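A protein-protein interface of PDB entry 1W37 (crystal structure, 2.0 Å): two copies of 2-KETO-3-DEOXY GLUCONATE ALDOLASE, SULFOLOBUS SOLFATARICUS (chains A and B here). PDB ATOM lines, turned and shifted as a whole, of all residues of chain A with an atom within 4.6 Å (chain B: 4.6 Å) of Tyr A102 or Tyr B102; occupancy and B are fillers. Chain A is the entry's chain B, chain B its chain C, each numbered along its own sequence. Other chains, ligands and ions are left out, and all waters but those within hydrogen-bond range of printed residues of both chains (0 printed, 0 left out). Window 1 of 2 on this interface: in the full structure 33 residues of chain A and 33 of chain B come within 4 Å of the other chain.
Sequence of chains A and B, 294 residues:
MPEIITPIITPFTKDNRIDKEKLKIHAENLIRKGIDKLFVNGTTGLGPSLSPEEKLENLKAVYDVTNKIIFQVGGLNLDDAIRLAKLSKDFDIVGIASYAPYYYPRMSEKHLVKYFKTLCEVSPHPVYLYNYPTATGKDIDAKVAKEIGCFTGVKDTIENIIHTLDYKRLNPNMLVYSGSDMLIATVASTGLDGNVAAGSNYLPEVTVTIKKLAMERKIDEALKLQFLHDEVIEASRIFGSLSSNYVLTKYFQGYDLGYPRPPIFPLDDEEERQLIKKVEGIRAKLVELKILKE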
ATOM      1  N   PRO A  48      -6.366 -21.417 -34.293  1.00  0.00           N
ATOM      2  CA  PRO A  48      -6.345 -21.171 -32.818  1.00  0.00           C
ATOM      3  C   PRO A  48      -6.226 -19.690 -32.465  1.00  0.00           C
ATOM      4  O   PRO A  48      -6.569 -19.308 -31.349  1.00  0.00           O
ATOM      5  CB  PRO A  48      -5.137 -21.983 -32.340  1.00  0.00           C
ATOM      6  CG  PRO A  48      -5.001 -23.097 -33.374  1.00  0.00           C
ATOM      7  CD  PRO A  48      -5.361 -22.419 -34.684  1.00  0.00           C
ATOM      8  N   GLY A  75     -12.191 -25.408 -30.247  1.00  0.00           N
ATOM      9  CA  GLY A  75     -11.595 -24.455 -29.319  1.00  0.00           C
ATOM     10  C   GLY A  75     -11.822 -24.924 -27.880  1.00  0.00           C
ATOM     11  O   GLY A  75     -12.312 -26.058 -27.652  1.00  0.00           O
ATOM     12  N   LEU A  76     -11.473 -24.088 -26.898  1.00  0.00           N
ATOM     13  CA  LEU A  76     -11.543 -24.468 -25.500  1.00  0.00           C
ATOM     14  C   LEU A  76     -12.814 -24.005 -24.804  1.00  0.00           C
ATOM     15  O   LEU A  76     -12.910 -24.100 -23.568  1.00  0.00           O
ATOM     16  CB  LEU A  76     -10.346 -23.872 -24.733  1.00  0.00           C
ATOM     17  CG  LEU A  76      -9.021 -24.545 -25.153  1.00  0.00           C
ATOM     18  CD1 LEU A  76      -7.757 -23.841 -24.581  1.00  0.00           C
ATOM     19  CD2 LEU A  76      -9.115 -26.063 -24.734  1.00  0.00           C
ATOM     20  N   TYR A  99      -9.713 -29.996 -34.023  1.00  0.00           N
ATOM     21  CA  TYR A  99      -8.588 -30.604 -33.290  1.00  0.00           C
ATOM     22  C   TYR A  99      -9.047 -30.861 -31.870  1.00  0.00           C
ATOM     23  O   TYR A  99     -10.130 -30.419 -31.436  1.00  0.00           O
ATOM     24  CB  TYR A  99      -7.327 -29.710 -33.346  1.00  0.00           C
ATOM     25  CG  TYR A  99      -7.601 -28.187 -33.478  1.00  0.00           C
ATOM     26  CD1 TYR A  99      -8.395 -27.511 -32.531  1.00  0.00           C
ATOM     27  CD2 TYR A  99      -7.092 -27.455 -34.546  1.00  0.00           C
ATOM     28  CE1 TYR A  99      -8.668 -26.147 -32.648  1.00  0.00           C
ATOM     29  CE2 TYR A  99      -7.356 -26.066 -34.669  1.00  0.00           C
ATOM     30  CZ  TYR A  99      -8.138 -25.432 -33.719  1.00  0.00           C
ATOM     31  OH  TYR A  99      -8.429 -24.068 -33.838  1.00  0.00           O
ATOM     32  N   ALA A 100      -8.227 -31.579 -31.135  1.00  0.00           N
ATOM     33  CA  ALA A 100      -8.467 -31.828 -29.743  1.00  0.00           C
ATOM     34  C   ALA A 100      -8.313 -30.552 -28.955  1.00  0.00           C
ATOM     35  O   ALA A 100      -7.625 -29.597 -29.379  1.00  0.00           O
ATOM     36  CB  ALA A 100      -7.493 -32.940 -29.226  1.00  0.00           C
ATOM     37  N   PRO A 101      -8.918 -30.528 -27.787  1.00  0.00           N
ATOM     38  CA  PRO A 101      -8.706 -29.397 -26.885  1.00  0.00           C
ATOM     39  C   PRO A 101      -7.214 -29.248 -26.641  1.00  0.00           C
ATOM     40  O   PRO A 101      -6.552 -30.212 -26.258  1.00  0.00           O
ATOM     41  CB  PRO A 101      -9.441 -29.814 -25.596  1.00  0.00           C
ATOM     42  CG  PRO A 101     -10.491 -30.822 -26.083  1.00  0.00           C
ATOM     43  CD  PRO A 101      -9.838 -31.560 -27.234  1.00  0.00           C
ATOM     44  N   TYR A 102      -6.677 -28.065 -26.898  1.00  0.00           N
ATOM     45  CA  TYR A 102      -5.223 -27.869 -26.839  1.00  0.00           C
ATOM     46  C   TYR A 102      -4.773 -27.272 -25.497  1.00  0.00           C
ATOM     47  O   TYR A 102      -5.597 -27.084 -24.593  1.00  0.00           O
ATOM     48  CB  TYR A 102      -4.783 -26.982 -27.987  1.00  0.00           C
ATOM     49  CG  TYR A 102      -5.637 -25.778 -28.269  1.00  0.00           C
ATOM     50  CD1 TYR A 102      -5.659 -24.673 -27.413  1.00  0.00           C
ATOM     51  CD2 TYR A 102      -6.363 -25.693 -29.451  1.00  0.00           C
ATOM     52  CE1 TYR A 102      -6.441 -23.537 -27.717  1.00  0.00           C
ATOM     53  CE2 TYR A 102      -7.160 -24.592 -29.742  1.00  0.00           C
ATOM     54  CZ  TYR A 102      -7.206 -23.530 -28.880  1.00  0.00           C
ATOM     55  OH  TYR A 102      -7.982 -22.442 -29.259  1.00  0.00           O
ATOM     56  N   TYR A 103      -3.473 -27.018 -25.363  1.00  0.00           N
ATOM     57  CA  TYR A 103      -2.872 -26.439 -24.142  1.00  0.00           C
ATOM     58  C   TYR A 103      -2.862 -27.364 -22.899  1.00  0.00           C
ATOM     59  O   TYR A 103      -1.791 -27.735 -22.419  1.00  0.00           O
ATOM     60  CB  TYR A 103      -3.509 -25.085 -23.796  1.00  0.00           C
ATOM     61  CG  TYR A 103      -2.827 -24.376 -22.613  1.00  0.00           C
ATOM     62  CD1 TYR A 103      -1.852 -23.403 -22.843  1.00  0.00           C
ATOM     63  CD2 TYR A 103      -3.129 -24.722 -21.300  1.00  0.00           C
ATOM     64  CE1 TYR A 103      -1.230 -22.741 -21.781  1.00  0.00           C
ATOM     65  CE2 TYR A 103      -2.485 -24.078 -20.197  1.00  0.00           C
ATOM     66  CZ  TYR A 103      -1.564 -23.075 -20.462  1.00  0.00           C
ATOM     67  OH  TYR A 103      -0.932 -22.461 -19.411  1.00  0.00           O
ATOM     68  N   TYR A 104      -4.036 -27.726 -22.366  1.00  0.00           N
ATOM     69  CA  TYR A 104      -4.061 -28.451 -21.094  1.00  0.00           C
ATOM     70  C   TYR A 104      -3.440 -29.836 -21.224  1.00  0.00           C
ATOM     71  O   TYR A 104      -3.889 -30.624 -22.011  1.00  0.00           O
ATOM     72  CB  TYR A 104      -5.491 -28.567 -20.527  1.00  0.00           C
ATOM     73  CG  TYR A 104      -6.167 -27.214 -20.379  1.00  0.00           C
ATOM     74  CD1 TYR A 104      -7.191 -26.812 -21.265  1.00  0.00           C
ATOM     75  CD2 TYR A 104      -5.828 -26.382 -19.343  1.00  0.00           C
ATOM     76  CE1 TYR A 104      -7.840 -25.567 -21.100  1.00  0.00           C
ATOM     77  CE2 TYR A 104      -6.421 -25.134 -19.194  1.00  0.00           C
ATOM     78  CZ  TYR A 104      -7.410 -24.733 -20.069  1.00  0.00           C
ATOM     79  OH  TYR A 104      -7.982 -23.508 -19.870  1.00  0.00           O
ATOM     80  N   THR A 136      -1.328 -29.872 -30.099  1.00  0.00           N
ATOM     81  CA  THR A 136      -2.380 -29.901 -29.054  1.00  0.00           C
ATOM     82  C   THR A 136      -1.997 -30.539 -27.750  1.00  0.00           C
ATOM     83  O   THR A 136      -2.731 -30.344 -26.751  1.00  0.00           O
ATOM     84  CB  THR A 136      -3.666 -30.680 -29.533  1.00  0.00           C
ATOM     85  OG1 THR A 136      -3.288 -32.024 -29.796  1.00  0.00           O
ATOM     86  CG2 THR A 136      -4.148 -30.158 -30.891  1.00  0.00           C
ATOM     87  N   PRO B  48      -6.565 -19.996 -20.740  1.00  0.00           N
ATOM     88  CA  PRO B  48      -6.736 -20.206 -22.186  1.00  0.00           C
ATOM     89  C   PRO B  48      -8.173 -20.459 -22.634  1.00  0.00           C
ATOM     90  O   PRO B  48      -8.457 -20.204 -23.798  1.00  0.00           O
ATOM     91  CB  PRO B  48      -5.848 -21.433 -22.468  1.00  0.00           C
ATOM     92  CG  PRO B  48      -4.826 -21.450 -21.317  1.00  0.00           C
ATOM     93  CD  PRO B  48      -5.624 -20.962 -20.139  1.00  0.00           C
ATOM     94  N   GLY B  75      -2.270 -14.599 -24.907  1.00  0.00           N
ATOM     95  CA  GLY B  75      -3.053 -15.420 -25.811  1.00  0.00           C
ATOM     96  C   GLY B  75      -2.517 -15.249 -27.229  1.00  0.00           C
ATOM     97  O   GLY B  75      -1.423 -14.679 -27.409  1.00  0.00           O
ATOM     98  N   LEU B  76      -3.296 -15.668 -28.235  1.00  0.00           N
ATOM     99  CA  LEU B  76      -2.759 -15.745 -29.590  1.00  0.00           C
ATOM    100  C   LEU B  76      -3.221 -14.619 -30.481  1.00  0.00           C
ATOM    101  O   LEU B  76      -3.024 -14.647 -31.701  1.00  0.00           O
ATOM    102  CB  LEU B  76      -3.146 -17.089 -30.209  1.00  0.00           C
ATOM    103  CG  LEU B  76      -2.543 -18.307 -29.491  1.00  0.00           C
ATOM    104  CD1 LEU B  76      -3.146 -19.600 -30.091  1.00  0.00           C
ATOM    105  CD2 LEU B  76      -1.040 -18.245 -29.717  1.00  0.00           C
ATOM    106  N   TYR B  99       1.937 -16.406 -20.287  1.00  0.00           N
ATOM    107  CA  TYR B  99       2.575 -17.566 -20.888  1.00  0.00           C
ATOM    108  C   TYR B  99       2.987 -17.272 -22.328  1.00  0.00           C
ATOM    109  O   TYR B  99       2.569 -16.264 -22.939  1.00  0.00           O
ATOM    110  CB  TYR B  99       1.671 -18.836 -20.795  1.00  0.00           C
ATOM    111  CG  TYR B  99       0.177 -18.598 -20.880  1.00  0.00           C
ATOM    112  CD1 TYR B  99      -0.388 -18.021 -21.993  1.00  0.00           C
ATOM    113  CD2 TYR B  99      -0.661 -18.970 -19.835  1.00  0.00           C
ATOM    114  CE1 TYR B  99      -1.800 -17.808 -22.097  1.00  0.00           C
ATOM    115  CE2 TYR B  99      -2.035 -18.781 -19.926  1.00  0.00           C
ATOM    116  CZ  TYR B  99      -2.592 -18.187 -21.044  1.00  0.00           C
ATOM    117  OH  TYR B  99      -3.967 -17.972 -21.094  1.00  0.00           O
ATOM    118  N   ALA B 100       3.842 -18.141 -22.869  1.00  0.00           N
ATOM    119  CA  ALA B 100       4.295 -18.005 -24.236  1.00  0.00           C
ATOM    120  C   ALA B 100       3.121 -18.346 -25.141  1.00  0.00           C
ATOM    121  O   ALA B 100       2.182 -19.069 -24.735  1.00  0.00           O
ATOM    122  CB  ALA B 100       5.507 -19.002 -24.529  1.00  0.00           C
ATOM    123  N   PRO B 101       3.160 -17.855 -26.379  1.00  0.00           N
ATOM    124  CA  PRO B 101       2.157 -18.242 -27.376  1.00  0.00           C
ATOM    125  C   PRO B 101       2.043 -19.776 -27.463  1.00  0.00           C
ATOM    126  O   PRO B 101       3.054 -20.462 -27.688  1.00  0.00           O
ATOM    127  CB  PRO B 101       2.721 -17.650 -28.688  1.00  0.00           C
ATOM    128  CG  PRO B 101       3.572 -16.460 -28.204  1.00  0.00           C
ATOM    129  CD  PRO B 101       4.203 -16.968 -26.930  1.00  0.00           C
ATOM    130  N   TYR B 102       0.847 -20.323 -27.236  1.00  0.00           N
ATOM    131  CA  TYR B 102       0.711 -21.774 -27.104  1.00  0.00           C
ATOM    132  C   TYR B 102       0.291 -22.394 -28.473  1.00  0.00           C
ATOM    133  O   TYR B 102       0.175 -21.646 -29.482  1.00  0.00           O
ATOM    134  CB  TYR B 102      -0.275 -22.103 -25.989  1.00  0.00           C
ATOM    135  CG  TYR B 102      -1.576 -21.291 -25.965  1.00  0.00           C
ATOM    136  CD1 TYR B 102      -2.593 -21.501 -26.882  1.00  0.00           C
ATOM    137  CD2 TYR B 102      -1.804 -20.388 -24.961  1.00  0.00           C
ATOM    138  CE1 TYR B 102      -3.799 -20.721 -26.826  1.00  0.00           C
ATOM    139  CE2 TYR B 102      -2.949 -19.638 -24.887  1.00  0.00           C
ATOM    140  CZ  TYR B 102      -3.946 -19.803 -25.803  1.00  0.00           C
ATOM    141  OH  TYR B 102      -5.084 -19.057 -25.601  1.00  0.00           O
ATOM    142  N   TYR B 103       0.067 -23.712 -28.491  1.00  0.00           N
ATOM    143  CA  TYR B 103      -0.347 -24.465 -29.721  1.00  0.00           C
ATOM    144  C   TYR B 103       0.717 -24.563 -30.792  1.00  0.00           C
ATOM    145  O   TYR B 103       1.192 -25.659 -31.056  1.00  0.00           O
ATOM    146  CB  TYR B 103      -1.597 -23.888 -30.374  1.00  0.00           C
ATOM    147  CG  TYR B 103      -2.172 -24.778 -31.516  1.00  0.00           C
ATOM    148  CD1 TYR B 103      -3.140 -25.767 -31.263  1.00  0.00           C
ATOM    149  CD2 TYR B 103      -1.743 -24.595 -32.831  1.00  0.00           C
ATOM    150  CE1 TYR B 103      -3.667 -26.557 -32.337  1.00  0.00           C
ATOM    151  CE2 TYR B 103      -2.253 -25.365 -33.903  1.00  0.00           C
ATOM    152  CZ  TYR B 103      -3.184 -26.348 -33.652  1.00  0.00           C
ATOM    153  OH  TYR B 103      -3.649 -27.076 -34.770  1.00  0.00           O
ATOM    154  N   TYR B 104       1.106 -23.440 -31.424  1.00  0.00           N
ATOM    155  CA  TYR B 104       1.942 -23.497 -32.643  1.00  0.00           C
ATOM    156  C   TYR B 104       3.350 -24.007 -32.357  1.00  0.00           C
ATOM    157  O   TYR B 104       4.066 -23.379 -31.554  1.00  0.00           O
ATOM    158  CB  TYR B 104       2.069 -22.123 -33.312  1.00  0.00           C
ATOM    159  CG  TYR B 104       0.746 -21.533 -33.687  1.00  0.00           C
ATOM    160  CD1 TYR B 104       0.236 -20.427 -33.026  1.00  0.00           C
ATOM    161  CD2 TYR B 104      -0.027 -22.117 -34.713  1.00  0.00           C
ATOM    162  CE1 TYR B 104      -1.027 -19.881 -33.384  1.00  0.00           C
ATOM    163  CE2 TYR B 104      -1.293 -21.583 -35.087  1.00  0.00           C
ATOM    164  CZ  TYR B 104      -1.777 -20.483 -34.444  1.00  0.00           C
ATOM    165  OH  TYR B 104      -2.991 -19.976 -34.822  1.00  0.00           O
ATOM    166  N   ALA B 135       2.574 -27.322 -21.443  1.00  0.00           N
ATOM    167  CA  ALA B 135       1.317 -26.766 -21.907  1.00  0.00           C
ATOM    168  C   ALA B 135       1.499 -26.002 -23.186  1.00  0.00           C
ATOM    169  O   ALA B 135       0.674 -26.099 -24.072  1.00  0.00           O
ATOM    170  CB  ALA B 135       0.700 -25.797 -20.803  1.00  0.00           C
ATOM    171  N   THR B 136       2.511 -25.152 -23.250  1.00  0.00           N
ATOM    172  CA  THR B 136       2.580 -24.219 -24.358  1.00  0.00           C
ATOM    173  C   THR B 136       3.338 -24.777 -25.539  1.00  0.00           C
ATOM    174  O   THR B 136       3.242 -24.217 -26.596  1.00  0.00           O
ATOM    175  CB  THR B 136       3.263 -22.896 -23.998  1.00  0.00           C
ATOM    176  OG1 THR B 136       4.630 -23.191 -23.649  1.00  0.00           O
ATOM    177  CG2 THR B 136       2.612 -22.201 -22.774  1.00  0.00           C
ATOM    178  N   LYS B 138       6.582 -24.616 -25.796  1.00  0.00           N
ATOM    179  CA  LYS B 138       7.922 -24.084 -25.872  1.00  0.00           C
ATOM    180  C   LYS B 138       8.427 -23.634 -24.495  1.00  0.00           C
ATOM    181  O   LYS B 138       7.666 -23.499 -23.546  1.00  0.00           O
ATOM    182  CB  LYS B 138       8.028 -23.014 -26.995  1.00  0.00           C
ATOM    183  CG  LYS B 138       7.216 -21.734 -26.716  1.00  0.00           C
ATOM    184  CD  LYS B 138       5.807 -21.960 -27.175  1.00  0.00           C
ATOM    185  CE  LYS B 138       5.700 -22.611 -28.626  1.00  0.00           C
ATOM    186  NZ  LYS B 138       4.237 -22.676 -28.996  1.00  0.00           N
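Hydrophobic or aromatic side chains of chain B within 4 Å of the printed part of chain A: Pro B48, Leu B76, Tyr B99, Tyr B102, Tyr B103, Tyr B104 and Ala B135. Printed residues of chain A that touch a printed residue of chain B: Pro A48, Leu A76, Tyr A99, Tyr A102, Tyr A103, Tyr A104 and Thr A136. Among the printed residues, 13 pairs touch across the chains.
Tyr A102 touches just these residues of chain B: Tyr B102 and Tyr B103. Of the printed residues of chain B, Thr A136 touches Tyr B103 (3.9 Å). Of the printed residues of chain A, Tyr B102 touches Tyr A102 and Tyr A103. Printed residues of chain A within 4 Å of Ala B135: Tyr A103 (3.3 Å). Lys B138 touches none of the printed residues of chain A.
O of Tyr A103 lies close to O of Ala B135, 3.4 Å away.
O of Pro A48 touches CD1 of Leu B76 (3.7 Å). CG of Pro A48 touches CE2 of Tyr B103 (3.6 Å). Pro A48 touches Tyr B104 (CD to OH, 3.4 Å). Pro B48 touches Leu A76. Tyr A102 touches Tyr B103. CD2 of Tyr A103 touches CG of Pro B48 (3.7 Å). Tyr A103 touches Tyr B99. CD2 of Tyr B102 touches CD1 of Tyr A103, at 3.7 Å. CD of Pro B48 touches OH of Tyr A104, 3.5 Å away. CG2 of Thr A136 touches CE1 of Tyr B103 (3.9 Å).
Pro A48 touches Tyr B103, and with the chains exchanged Tyr A103 touches Pro B48. Tyr A99 touches Tyr B103, and with the chains exchanged Tyr A103 touches Tyr B99. Tyr A102 touches Tyr B103, and with the chains exchanged Tyr A103 touches Tyr B102. Thr A136 touches Tyr B103, but with the chains exchanged Tyr A103 does not touch Thr B136 (4.005 Å). Of the 13 pairs that touch across the chains among the printed residues, 11 have their exchanged pair printed and touching as well.
O of Tyr B104 sits at hydrogen-bond distance from NZ of Lys B138 (2.7 Å).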
